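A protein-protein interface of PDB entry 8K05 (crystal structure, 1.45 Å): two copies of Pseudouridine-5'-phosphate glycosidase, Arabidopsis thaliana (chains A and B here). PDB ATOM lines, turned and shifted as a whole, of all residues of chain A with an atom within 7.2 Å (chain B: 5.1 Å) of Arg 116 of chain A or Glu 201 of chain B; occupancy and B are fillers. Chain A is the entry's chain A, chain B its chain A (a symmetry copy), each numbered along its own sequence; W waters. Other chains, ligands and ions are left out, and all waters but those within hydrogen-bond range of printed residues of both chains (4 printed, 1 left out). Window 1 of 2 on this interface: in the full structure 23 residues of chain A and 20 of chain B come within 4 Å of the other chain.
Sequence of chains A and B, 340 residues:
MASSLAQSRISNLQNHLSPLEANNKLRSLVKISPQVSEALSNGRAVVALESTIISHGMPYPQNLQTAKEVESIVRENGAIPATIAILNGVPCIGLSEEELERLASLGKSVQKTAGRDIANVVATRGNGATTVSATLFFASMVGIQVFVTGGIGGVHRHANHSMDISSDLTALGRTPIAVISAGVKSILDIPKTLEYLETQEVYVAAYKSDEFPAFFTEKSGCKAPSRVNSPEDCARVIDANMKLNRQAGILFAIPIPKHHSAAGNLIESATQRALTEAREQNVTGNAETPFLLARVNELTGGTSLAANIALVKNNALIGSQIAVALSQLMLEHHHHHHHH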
ATOM      1  N   THR A 113     -19.504 -19.141 -18.703  1.00  0.00           N
ATOM      2  CA  THR A 113     -19.842 -19.954 -17.543  1.00  0.00           C
ATOM      3  C   THR A 113     -18.613 -20.646 -16.956  1.00  0.00           C
ATOM      4  O   THR A 113     -18.115 -21.623 -17.513  1.00  0.00           O
ATOM      5  CB  THR A 113     -20.902 -21.014 -17.908  1.00  0.00           C
ATOM      6  OG1 THR A 113     -22.046 -20.363 -18.488  1.00  0.00           O
ATOM      7  CG2 THR A 113     -21.341 -21.793 -16.685  1.00  0.00           C
ATOM      8  N   ALA A 114     -18.109 -20.111 -15.849  1.00  0.00           N
ATOM      9  CA  ALA A 114     -17.052 -20.780 -15.097  1.00  0.00           C
ATOM     10  C   ALA A 114     -17.660 -21.907 -14.268  1.00  0.00           C
ATOM     11  O   ALA A 114     -18.880 -22.033 -14.172  1.00  0.00           O
ATOM     12  CB  ALA A 114     -16.313 -19.779 -14.208  1.00  0.00           C
ATOM     13  N   GLY A 115     -16.823 -22.745 -13.664  1.00  0.00           N
ATOM     14  CA  GLY A 115     -17.355 -23.827 -12.855  1.00  0.00           C
ATOM     15  C   GLY A 115     -18.352 -23.363 -11.803  1.00  0.00           C
ATOM     16  O   GLY A 115     -19.394 -23.990 -11.607  1.00  0.00           O
ATOM     17  N   ARG A 116     -18.023 -22.265 -11.125  1.00  0.00           N
ATOM     18  CA  ARG A 116     -18.894 -21.763 -10.066  1.00  0.00           C
ATOM     19  C   ARG A 116     -20.222 -21.209 -10.588  1.00  0.00           C
ATOM     20  O   ARG A 116     -21.136 -20.977  -9.794  1.00  0.00           O
ATOM     21  CB  ARG A 116     -18.174 -20.680  -9.263  1.00  0.00           C
ATOM     22  CG  ARG A 116     -17.880 -19.458 -10.073  1.00  0.00           C
ATOM     23  CD  ARG A 116     -17.073 -18.391  -9.322  1.00  0.00           C
ATOM     24  NE  ARG A 116     -16.737 -17.381 -10.323  1.00  0.00           N
ATOM     25  CZ  ARG A 116     -15.605 -17.363 -11.016  1.00  0.00           C
ATOM     26  NH1 ARG A 116     -14.644 -18.246 -10.751  1.00  0.00           N
ATOM     27  NH2 ARG A 116     -15.418 -16.445 -11.955  1.00  0.00           N
ATOM     28  N   ASP A 117     -20.337 -21.000 -11.901  1.00  0.00           N
ATOM     29  CA  ASP A 117     -21.564 -20.476 -12.511  1.00  0.00           C
ATOM     30  C   ASP A 117     -22.510 -21.547 -13.017  1.00  0.00           C
ATOM     31  O   ASP A 117     -23.645 -21.237 -13.384  1.00  0.00           O
ATOM     32  CB  ASP A 117     -21.217 -19.562 -13.684  1.00  0.00           C
ATOM     33  CG  ASP A 117     -20.359 -18.399 -13.275  1.00  0.00           C
ATOM     34  OD1 ASP A 117     -20.721 -17.718 -12.287  1.00  0.00           O
ATOM     35  OD2 ASP A 117     -19.329 -18.165 -13.923  1.00  0.00           O
ATOM     36  N   ILE A 118     -22.059 -22.794 -13.065  1.00  0.00           N
ATOM     37  CA  ILE A 118     -22.856 -23.846 -13.692  1.00  0.00           C
ATOM     38  C   ILE A 118     -24.234 -23.994 -13.048  1.00  0.00           C
ATOM     39  O   ILE A 118     -25.246 -24.013 -13.755  1.00  0.00           O
ATOM     40  CB  ILE A 118     -22.139 -25.208 -13.642  1.00  0.00           C
ATOM     41  CG1 ILE A 118     -20.824 -25.138 -14.431  1.00  0.00           C
ATOM     42  CG2 ILE A 118     -23.057 -26.311 -14.178  1.00  0.00           C
ATOM     43  CD1 ILE A 118     -19.927 -26.341 -14.195  1.00  0.00           C
ATOM     44  N   ALA A 119     -24.280 -24.081 -11.722  1.00  0.00           N
ATOM     45  CA  ALA A 119     -25.545 -24.316 -11.035  1.00  0.00           C
ATOM     46  C   ALA A 119     -26.532 -23.191 -11.320  1.00  0.00           C
ATOM     47  O   ALA A 119     -27.718 -23.452 -11.522  1.00  0.00           O
ATOM     48  CB  ALA A 119     -25.323 -24.474  -9.531  1.00  0.00           C
ATOM     49  N   ASN A 120     -26.051 -21.953 -11.367  1.00  0.00           N
ATOM     50  CA  ASN A 120     -26.927 -20.816 -11.635  1.00  0.00           C
ATOM     51  C   ASN A 120     -27.459 -20.846 -13.070  1.00  0.00           C
ATOM     52  O   ASN A 120     -28.640 -20.582 -13.302  1.00  0.00           O
ATOM     53  CB  ASN A 120     -26.188 -19.506 -11.366  1.00  0.00           C
ATOM     54  CG  ASN A 120     -27.098 -18.296 -11.444  1.00  0.00           C
ATOM     55  OD1 ASN A 120     -28.220 -18.317 -10.937  1.00  0.00           O
ATOM     56  ND2 ASN A 120     -26.617 -17.235 -12.074  1.00  0.00           N
ATOM     57  N   VAL A 121     -26.612 -21.197 -14.031  1.00  0.00           N
ATOM     58  CA  VAL A 121     -27.066 -21.278 -15.419  1.00  0.00           C
ATOM     59  C   VAL A 121     -28.097 -22.400 -15.576  1.00  0.00           C
ATOM     60  O   VAL A 121     -29.109 -22.228 -16.267  1.00  0.00           O
ATOM     61  CB  VAL A 121     -25.881 -21.488 -16.393  1.00  0.00           C
ATOM     62  CG1 VAL A 121     -26.404 -21.647 -17.825  1.00  0.00           C
ATOM     63  CG2 VAL A 121     -24.948 -20.315 -16.326  1.00  0.00           C
ATOM     64  N   THR A 131     -16.213 -22.327 -19.633  1.00  0.00           N
ATOM     65  CA  THR A 131     -14.783 -22.017 -19.613  1.00  0.00           C
ATOM     66  C   THR A 131     -13.973 -23.270 -19.309  1.00  0.00           C
ATOM     67  O   THR A 131     -14.537 -24.358 -19.184  1.00  0.00           O
ATOM     68  CB  THR A 131     -14.449 -20.964 -18.551  1.00  0.00           C
ATOM     69  OG1 THR A 131     -14.715 -21.518 -17.259  1.00  0.00           O
ATOM     70  CG2 THR A 131     -15.299 -19.709 -18.752  1.00  0.00           C
ATOM     71  N   SER A 133     -12.532 -24.131 -16.455  1.00  0.00           N
ATOM     72  CA  SER A 133     -12.907 -24.718 -15.176  1.00  0.00           C
ATOM     73  C   SER A 133     -14.235 -25.488 -15.256  1.00  0.00           C
ATOM     74  O   SER A 133     -14.375 -26.555 -14.665  1.00  0.00           O
ATOM     75  CB  SER A 133     -12.986 -23.645 -14.079  1.00  0.00           C
ATOM     76  OG  SER A 133     -14.011 -22.691 -14.345  1.00  0.00           O
ATOM     77  N   ALA A 134     -15.203 -24.957 -15.997  1.00  0.00           N
ATOM     78  CA  ALA A 134     -16.489 -25.633 -16.107  1.00  0.00           C
ATOM     79  C   ALA A 134     -16.422 -26.848 -17.027  1.00  0.00           C
ATOM     80  O   ALA A 134     -17.033 -27.893 -16.760  1.00  0.00           O
ATOM     81  CB  ALA A 134     -17.546 -24.658 -16.603  1.00  0.00           C
ATOM     82  N   LEU A 136     -13.791 -28.713 -17.710  1.00  0.00           N
ATOM     83  CA  LEU A 136     -13.059 -29.840 -17.167  1.00  0.00           C
ATOM     84  C   LEU A 136     -13.888 -30.540 -16.070  1.00  0.00           C
ATOM     85  O   LEU A 136     -13.793 -31.762 -15.918  1.00  0.00           O
ATOM     86  CB  LEU A 136     -11.670 -29.398 -16.705  1.00  0.00           C
ATOM     87  CG  LEU A 136     -11.441 -28.527 -15.486  1.00  0.00           C
ATOM     88  CD1 LEU A 136     -11.523 -29.364 -14.247  1.00  0.00           C
ATOM     89  CD2 LEU A 136     -10.058 -27.854 -15.558  1.00  0.00           C
ATOM     90  N   PHE A 137     -14.752 -29.807 -15.361  1.00  0.00           N
ATOM     91  CA  PHE A 137     -15.675 -30.446 -14.425  1.00  0.00           C
ATOM     92  C   PHE A 137     -16.564 -31.463 -15.150  1.00  0.00           C
ATOM     93  O   PHE A 137     -16.661 -32.626 -14.739  1.00  0.00           O
ATOM     94  CB  PHE A 137     -16.554 -29.405 -13.703  1.00  0.00           C
ATOM     95  CG  PHE A 137     -17.705 -30.007 -12.945  1.00  0.00           C
ATOM     96  CD1 PHE A 137     -17.490 -30.641 -11.728  1.00  0.00           C
ATOM     97  CD2 PHE A 137     -19.001 -29.959 -13.455  1.00  0.00           C
ATOM     98  CE1 PHE A 137     -18.537 -31.218 -11.030  1.00  0.00           C
ATOM     99  CE2 PHE A 137     -20.056 -30.538 -12.767  1.00  0.00           C
ATOM    100  CZ  PHE A 137     -19.825 -31.171 -11.550  1.00  0.00           C
ATOM    101  N   ILE A 165      -7.005 -14.432  -9.631  1.00  0.00           N
ATOM    102  CA  ILE A 165      -6.399 -15.689 -10.080  1.00  0.00           C
ATOM    103  C   ILE A 165      -7.480 -16.593 -10.652  1.00  0.00           C
ATOM    104  O   ILE A 165      -8.500 -16.833 -10.007  1.00  0.00           O
ATOM    105  CB  ILE A 165      -5.681 -16.407  -8.921  1.00  0.00           C
ATOM    106  CG1 ILE A 165      -4.561 -15.521  -8.364  1.00  0.00           C
ATOM    107  CG2 ILE A 165      -5.128 -17.768  -9.381  1.00  0.00           C
ATOM    108  CD1 ILE A 165      -3.872 -16.082  -7.142  1.00  0.00           C
ATOM    109  N   SER A 166      -7.272 -17.109 -11.858  1.00  0.00           N
ATOM    110  CA  SER A 166      -8.302 -17.909 -12.497  1.00  0.00           C
ATOM    111  C   SER A 166      -8.615 -19.200 -11.744  1.00  0.00           C
ATOM    112  O   SER A 166      -7.701 -19.925 -11.330  1.00  0.00           O
ATOM    113  CB  SER A 166      -7.887 -18.267 -13.927  1.00  0.00           C
ATOM    114  OG  SER A 166      -8.881 -19.067 -14.527  1.00  0.00           O
ATOM    115  N   SER A 167      -9.905 -19.491 -11.603  1.00  0.00           N
ATOM    116  CA  SER A 167     -10.338 -20.770 -11.033  1.00  0.00           C
ATOM    117  C   SER A 167      -9.929 -21.945 -11.901  1.00  0.00           C
ATOM    118  O   SER A 167     -10.027 -23.080 -11.455  1.00  0.00           O
ATOM    119  CB  SER A 167     -11.859 -20.809 -10.819  1.00  0.00           C
ATOM    120  OG  SER A 167     -12.559 -20.750 -12.054  1.00  0.00           O
ATOM    121  N   ASP A 168      -9.483 -21.695 -13.135  1.00  0.00           N
ATOM    122  CA  ASP A 168      -8.939 -22.782 -13.953  1.00  0.00           C
ATOM    123  C   ASP A 168      -7.829 -23.519 -13.219  1.00  0.00           C
ATOM    124  O   ASP A 168      -7.705 -24.744 -13.340  1.00  0.00           O
ATOM    125  CB  ASP A 168      -8.374 -22.266 -15.285  1.00  0.00           C
ATOM    126  CG  ASP A 168      -9.435 -21.740 -16.226  1.00  0.00           C
ATOM    127  OD1 ASP A 168     -10.643 -21.879 -15.942  1.00  0.00           O
ATOM    128  OD2 ASP A 168      -9.033 -21.193 -17.289  1.00  0.00           O
ATOM    129  N   THR A 170      -7.182 -23.759  -9.848  1.00  0.00           N
ATOM    130  CA  THR A 170      -7.761 -24.533  -8.754  1.00  0.00           C
ATOM    131  C   THR A 170      -8.437 -25.792  -9.276  1.00  0.00           C
ATOM    132  O   THR A 170      -8.264 -26.906  -8.744  1.00  0.00           O
ATOM    133  CB  THR A 170      -8.804 -23.673  -7.999  1.00  0.00           C
ATOM    134  OG1 THR A 170      -8.171 -22.457  -7.571  1.00  0.00           O
ATOM    135  CG2 THR A 170      -9.357 -24.425  -6.800  1.00  0.00           C
ATOM    136  N   ALA A 171      -9.234 -25.609 -10.320  1.00  0.00           N
ATOM    137  CA  ALA A 171     -10.003 -26.704 -10.865  1.00  0.00           C
ATOM    138  C   ALA A 171      -9.069 -27.813 -11.343  1.00  0.00           C
ATOM    139  O   ALA A 171      -9.285 -28.997 -11.042  1.00  0.00           O
ATOM    140  CB  ALA A 171     -10.895 -26.210 -11.997  1.00  0.00           C
ATOM    141  N   LEU A 172      -8.016 -27.436 -12.055  1.00  0.00           N
ATOM    142  CA  LEU A 172      -7.102 -28.448 -12.569  1.00  0.00           C
ATOM    143  C   LEU A 172      -6.337 -29.127 -11.417  1.00  0.00           C
ATOM    144  O   LEU A 172      -6.027 -30.330 -11.489  1.00  0.00           O
ATOM    145  CB  LEU A 172      -6.151 -27.828 -13.590  1.00  0.00           C
ATOM    146  CG  LEU A 172      -5.313 -28.824 -14.381  1.00  0.00           C
ATOM    147  CD1 LEU A 172      -6.161 -29.916 -15.012  1.00  0.00           C
ATOM    148  CD2 LEU A 172      -4.532 -28.069 -15.449  1.00  0.00           C
ATOM    149  N   ARG A 174      -7.566 -30.058  -8.710  1.00  0.00           N
ATOM    150  CA  ARG A 174      -8.354 -31.081  -8.037  1.00  0.00           C
ATOM    151  C   ARG A 174      -9.253 -31.881  -8.980  1.00  0.00           C
ATOM    152  O   ARG A 174     -10.224 -32.500  -8.557  1.00  0.00           O
ATOM    153  CB  ARG A 174      -9.160 -30.459  -6.895  1.00  0.00           C
ATOM    154  CG  ARG A 174     -10.115 -29.393  -7.297  1.00  0.00           C
ATOM    155  CD  ARG A 174     -10.604 -28.707  -6.035  1.00  0.00           C
ATOM    156  NE  ARG A 174     -11.595 -27.678  -6.299  1.00  0.00           N
ATOM    157  CZ  ARG A 174     -11.877 -26.684  -5.458  1.00  0.00           C
ATOM    158  NH1 ARG A 174     -12.811 -25.801  -5.773  1.00  0.00           N
ATOM    159  NH2 ARG A 174     -11.223 -26.570  -4.307  1.00  0.00           N
ATOM    160  N   THR A 175      -8.879 -31.917 -10.254  1.00  0.00           N
ATOM    161  CA  THR A 175      -9.611 -32.717 -11.224  1.00  0.00           C
ATOM    162  C   THR A 175      -8.617 -33.538 -12.040  1.00  0.00           C
ATOM    163  O   THR A 175      -7.758 -32.967 -12.701  1.00  0.00           O
ATOM    164  CB  THR A 175     -10.429 -31.832 -12.150  1.00  0.00           C
ATOM    165  OG1 THR A 175     -11.178 -30.885 -11.375  1.00  0.00           O
ATOM    166  CG2 THR A 175     -11.387 -32.668 -12.961  1.00  0.00           C
ATOM    167  N   LEU B 197     -12.723 -16.089  -3.221  1.00  0.00           N
ATOM    168  CA  LEU B 197     -13.886 -16.954  -3.399  1.00  0.00           C
ATOM    169  C   LEU B 197     -14.087 -17.381  -4.860  1.00  0.00           C
ATOM    170  O   LEU B 197     -14.447 -18.534  -5.120  1.00  0.00           O
ATOM    171  CB  LEU B 197     -15.141 -16.252  -2.857  1.00  0.00           C
ATOM    172  CG  LEU B 197     -15.248 -16.217  -1.331  1.00  0.00           C
ATOM    173  CD1 LEU B 197     -16.301 -15.186  -0.951  1.00  0.00           C
ATOM    174  CD2 LEU B 197     -15.607 -17.602  -0.808  1.00  0.00           C
ATOM    175  N   GLU B 198     -13.865 -16.469  -5.812  1.00  0.00           N
ATOM    176  CA  GLU B 198     -13.926 -16.839  -7.234  1.00  0.00           C
ATOM    177  C   GLU B 198     -12.921 -17.952  -7.545  1.00  0.00           C
ATOM    178  O   GLU B 198     -13.263 -18.945  -8.198  1.00  0.00           O
ATOM    179  CB  GLU B 198     -13.648 -15.632  -8.137  1.00  0.00           C
ATOM    180  CG  GLU B 198     -14.787 -14.613  -8.219  1.00  0.00           C
ATOM    181  CD  GLU B 198     -14.672 -13.699  -9.433  1.00  0.00           C
ATOM    182  OE1 GLU B 198     -13.748 -13.888 -10.247  1.00  0.00           O
ATOM    183  OE2 GLU B 198     -15.538 -12.803  -9.587  1.00  0.00           O
ATOM    184  N   THR B 199     -11.696 -17.782  -7.071  1.00  0.00           N
ATOM    185  CA  THR B 199     -10.633 -18.746  -7.342  1.00  0.00           C
ATOM    186  C   THR B 199     -10.950 -20.116  -6.729  1.00  0.00           C
ATOM    187  O   THR B 199     -10.602 -21.146  -7.308  1.00  0.00           O
ATOM    188  CB  THR B 199      -9.310 -18.214  -6.824  1.00  0.00           C
ATOM    189  OG1 THR B 199      -9.103 -16.895  -7.354  1.00  0.00           O
ATOM    190  CG2 THR B 199      -8.154 -19.115  -7.252  1.00  0.00           C
ATOM    191  N   GLN B 200     -11.645 -20.124  -5.592  1.00  0.00           N
ATOM    192  CA  GLN B 200     -12.031 -21.362  -4.909  1.00  0.00           C
ATOM    193  C   GLN B 200     -13.263 -22.025  -5.512  1.00  0.00           C
ATOM    194  O   GLN B 200     -13.662 -23.107  -5.064  1.00  0.00           O
ATOM    195  CB  GLN B 200     -12.284 -21.089  -3.414  1.00  0.00           C
ATOM    196  CG  GLN B 200     -11.039 -20.717  -2.634  1.00  0.00           C
ATOM    197  CD  GLN B 200      -9.987 -21.820  -2.653  1.00  0.00           C
ATOM    198  OE1 GLN B 200     -10.263 -22.962  -2.282  1.00  0.00           O
ATOM    199  NE2 GLN B 200      -8.791 -21.484  -3.101  1.00  0.00           N
ATOM    200  N   GLU B 201     -13.864 -21.377  -6.507  1.00  0.00           N
ATOM    201  CA  GLU B 201     -15.035 -21.872  -7.230  1.00  0.00           C
ATOM    202  C   GLU B 201     -16.308 -21.827  -6.390  1.00  0.00           C
ATOM    203  O   GLU B 201     -17.229 -22.616  -6.605  1.00  0.00           O
ATOM    204  CB  GLU B 201     -14.816 -23.302  -7.733  1.00  0.00           C
ATOM    205  CG  GLU B 201     -13.594 -23.456  -8.635  1.00  0.00           C
ATOM    206  CD  GLU B 201     -13.762 -24.624  -9.576  1.00  0.00           C
ATOM    207  OE1 GLU B 201     -13.201 -25.697  -9.285  1.00  0.00           O
ATOM    208  OE2 GLU B 201     -14.482 -24.456 -10.578  1.00  0.00           O
ATOM    209  N   VAL B 202     -16.373 -20.861  -5.480  1.00  0.00           N
ATOM    210  CA  VAL B 202     -17.581 -20.629  -4.684  1.00  0.00           C
ATOM    211  C   VAL B 202     -18.509 -19.686  -5.432  1.00  0.00           C
ATOM    212  O   VAL B 202     -18.104 -18.599  -5.828  1.00  0.00           O
ATOM    213  CB  VAL B 202     -17.247 -20.035  -3.317  1.00  0.00           C
ATOM    214  CG1 VAL B 202     -18.536 -19.679  -2.543  1.00  0.00           C
ATOM    215  CG2 VAL B 202     -16.383 -20.999  -2.512  1.00  0.00           C
ATOM    216  N   TYR B 203     -19.745 -20.121  -5.659  1.00  0.00           N
ATOM    217  CA  TYR B 203     -20.755 -19.249  -6.239  1.00  0.00           C
ATOM    218  C   TYR B 203     -21.194 -18.236  -5.181  1.00  0.00           C
ATOM    219  O   TYR B 203     -21.625 -18.630  -4.094  1.00  0.00           O
ATOM    220  CB  TYR B 203     -21.954 -20.055  -6.739  1.00  0.00           C
ATOM    221  CG  TYR B 203     -23.084 -19.193  -7.243  1.00  0.00           C
ATOM    222  CD1 TYR B 203     -22.941 -18.415  -8.393  1.00  0.00           C
ATOM    223  CD2 TYR B 203     -24.297 -19.153  -6.570  1.00  0.00           C
ATOM    224  CE1 TYR B 203     -23.982 -17.612  -8.860  1.00  0.00           C
ATOM    225  CE2 TYR B 203     -25.347 -18.357  -7.032  1.00  0.00           C
ATOM    226  CZ  TYR B 203     -25.178 -17.595  -8.167  1.00  0.00           C
ATOM    227  OH  TYR B 203     -26.232 -16.806  -8.594  1.00  0.00           O
ATOM    228  N   ARG B 246     -21.445 -31.183  -7.531  1.00  0.00           N
ATOM    229  CA  ARG B 246     -20.296 -30.286  -7.378  1.00  0.00           C
ATOM    230  C   ARG B 246     -19.805 -30.327  -5.941  1.00  0.00           C
ATOM    231  O   ARG B 246     -20.608 -30.417  -5.018  1.00  0.00           O
ATOM    232  CB  ARG B 246     -20.651 -28.840  -7.733  1.00  0.00           C
ATOM    233  CG  ARG B 246     -21.035 -28.580  -9.177  1.00  0.00           C
ATOM    234  CD  ARG B 246     -19.881 -28.002 -10.005  1.00  0.00           C
ATOM    235  NE  ARG B 246     -19.254 -26.776  -9.486  1.00  0.00           N
ATOM    236  CZ  ARG B 246     -18.024 -26.375  -9.832  1.00  0.00           C
ATOM    237  NH1 ARG B 246     -17.522 -25.258  -9.314  1.00  0.00           N
ATOM    238  NH2 ARG B 246     -17.282 -27.086 -10.698  1.00  0.00           N
ATOM    239  N   ALA B 248     -18.012 -27.871  -4.445  1.00  0.00           N
ATOM    240  CA  ALA B 248     -17.840 -26.521  -3.921  1.00  0.00           C
ATOM    241  C   ALA B 248     -19.187 -25.963  -3.508  1.00  0.00           C
ATOM    242  O   ALA B 248     -20.231 -26.371  -4.035  1.00  0.00           O
ATOM    243  CB  ALA B 248     -17.189 -25.609  -4.953  1.00  0.00           C
ATOM    244  N   GLY B 249     -19.154 -25.031  -2.560  1.00  0.00           N
ATOM    245  CA  GLY B 249     -20.369 -24.480  -1.988  1.00  0.00           C
ATOM    246  C   GLY B 249     -20.770 -23.122  -2.519  1.00  0.00           C
ATOM    247  O   GLY B 249     -20.279 -22.628  -3.534  1.00  0.00           O
HETATM  248  O   HOH W   1     -15.159 -21.761 -11.113  1.00  0.00           O
HETATM  249  O   HOH W   2     -14.566 -27.014 -11.837  1.00  0.00           O
HETATM  250  O   HOH W   3     -11.291 -25.050  -1.370  1.00  0.00           O
HETATM  251  O   HOH W   4      -9.882 -14.322  -8.548  1.00  0.00           O
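NH1 of Arg 174 of chain A is in salt-bridge range of OE1 of Glu 201 of chain B.
NH2 of Arg 116 of chain A lies within salt-bridge range of OE1 of Glu 198 of chain B (3.5 Å).
The backbone carbonyl oxygen of Ile 165 of chain A lies within hydrogen-bond range of the side-chain hydroxyl of Thr 199 of chain B, at 2.7 Å.
OH of Tyr 203 of chain B lies close to OD1 of Asn 120 of chain A (3.4 Å).
The backbone carbonyl oxygen (O) of Gly 115 of chain A lies within hydrogen-bond range of the guanidinium group (NH1) of Arg 246 of chain B (3.2 Å).
The guanidinium group of Arg 174 of chain A is in hydrogen-bond range of the backbone carbonyl oxygen of Gln 200 of chain B (2.9 Å).
The side-chain hydroxyl of Thr 170 of chain A is in hydrogen-bond range of the backbone carbonyl oxygen of Thr 199 of chain B.
O of Gly 249 of chain B is in hydrogen-bond range of N of Tyr 203 of chain B (3.3 Å).
The backbone NH of Ser 133 of chain A lies within hydrogen-bond range of the side-chain carboxylate of Asp 168 of chain A, 3.0 Å away.
The backbone carbonyl oxygen of Leu 197 of chain B sits at hydrogen-bond distance from the backbone NH of Val 202 of chain B (3.0 Å).
OG1 of Thr 175 of chain A sits at hydrogen-bond distance from O of Ala 171 of chain A (2.7 Å).
OE2 of Glu 201 of chain B is in salt-bridge range of NH1 of Arg 246 of chain B (3.4 Å).
The backbone NH (N) of Gly 115 of chain A sits at hydrogen-bond distance from the side-chain hydroxyl (OG) of Ser 133 of chain A.
Gly 115 of chain A touches Glu 201 of chain B.
CB of Arg 116 of chain A touches O of Glu 201 of chain B, 3.4 Å away.
Arg 116 of chain A touches Tyr 203 of chain B (O to CB, 3.3 Å).
Arg 116 of chain A touches Arg 246 of chain B.
Glu 201 of chain B touches Ser 133 of chain A.
CZ of Phe 137 of chain A touches CD of Arg 246 of chain B, 3.5 Å away.
O of Glu 198 of chain B touches CB of Ser 167 of chain A (3.5 Å).
Ser 167 of chain A touches Thr 199 of chain B (CB to O, 3.7 Å).
Glu 201 of chain B touches Ser 167 of chain A (CG to CB, 3.8 Å).
CB of Ala 171 of chain A touches OE1 of Glu 201 of chain B (3.6 Å).
Printed residues of chain B within 4 Å of Gly 115 of chain A: Glu 201 and Arg 246.
Printed residues of chain B within 4 Å of Arg 174 of chain A: Gln 200 and Glu 201.
Glu 201 of chain B touches just these residues of chain A: Gly 115, Arg 116, Ser 133, Ser 167, Ala 171 and Arg 174.
Of the printed residues of chain A, Val 202 of chain B touches Arg 116.
Of the printed residues of chain A, Arg 246 of chain B touches Gly 115, Arg 116 and Phe 137.
The nearest residue of chain A that does not touch Glu 201 of chain B is Thr 170 of chain A (4.7 Å).
Hydrophobic or aromatic side chains of chain B that line the printed part of chain A: Tyr 203.
Printed residues of chain A that touch a printed residue of chain B: Gly 115, Arg 116, Asn 120, Ser 133, Phe 137, Ile 165, Ser 167, Thr 170, Ala 171 and Arg 174.
Hydrophobic or aromatic side chains of chain A that line the printed part of chain B: Phe 137, Ile 165 and Ala 171.
No position is printed for both chains.
Of the 18 pairs that touch across the chains among the printed residues, none has its exchanged pair printed and touching as well.
Water W3 bridges OE1 of Gln 200 of chain B (2.5 Å) and NH2 of Arg 174 of chain A (3.3 Å).
Water W1 lies within hydrogen-bond range of OE2 of Glu 201 of chain B (2.8 Å), N of Arg 116 of chain A (2.9 Å), OG of Ser 167 of chain A (2.9 Å) and N of Gly 115 of chain A (3.2 Å).
Water W2 lies within hydrogen-bond range of the side-chain carboxylate of Glu 201 of chain B, the backbone carbonyl oxygen of Ser 133 of chain A and the guanidinium group of Arg 246 of chain B.
Water W4 bridges OG1 of Thr 199 of chain B (2.9 Å) and N of Ile 165 of chain A (3.1 Å).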
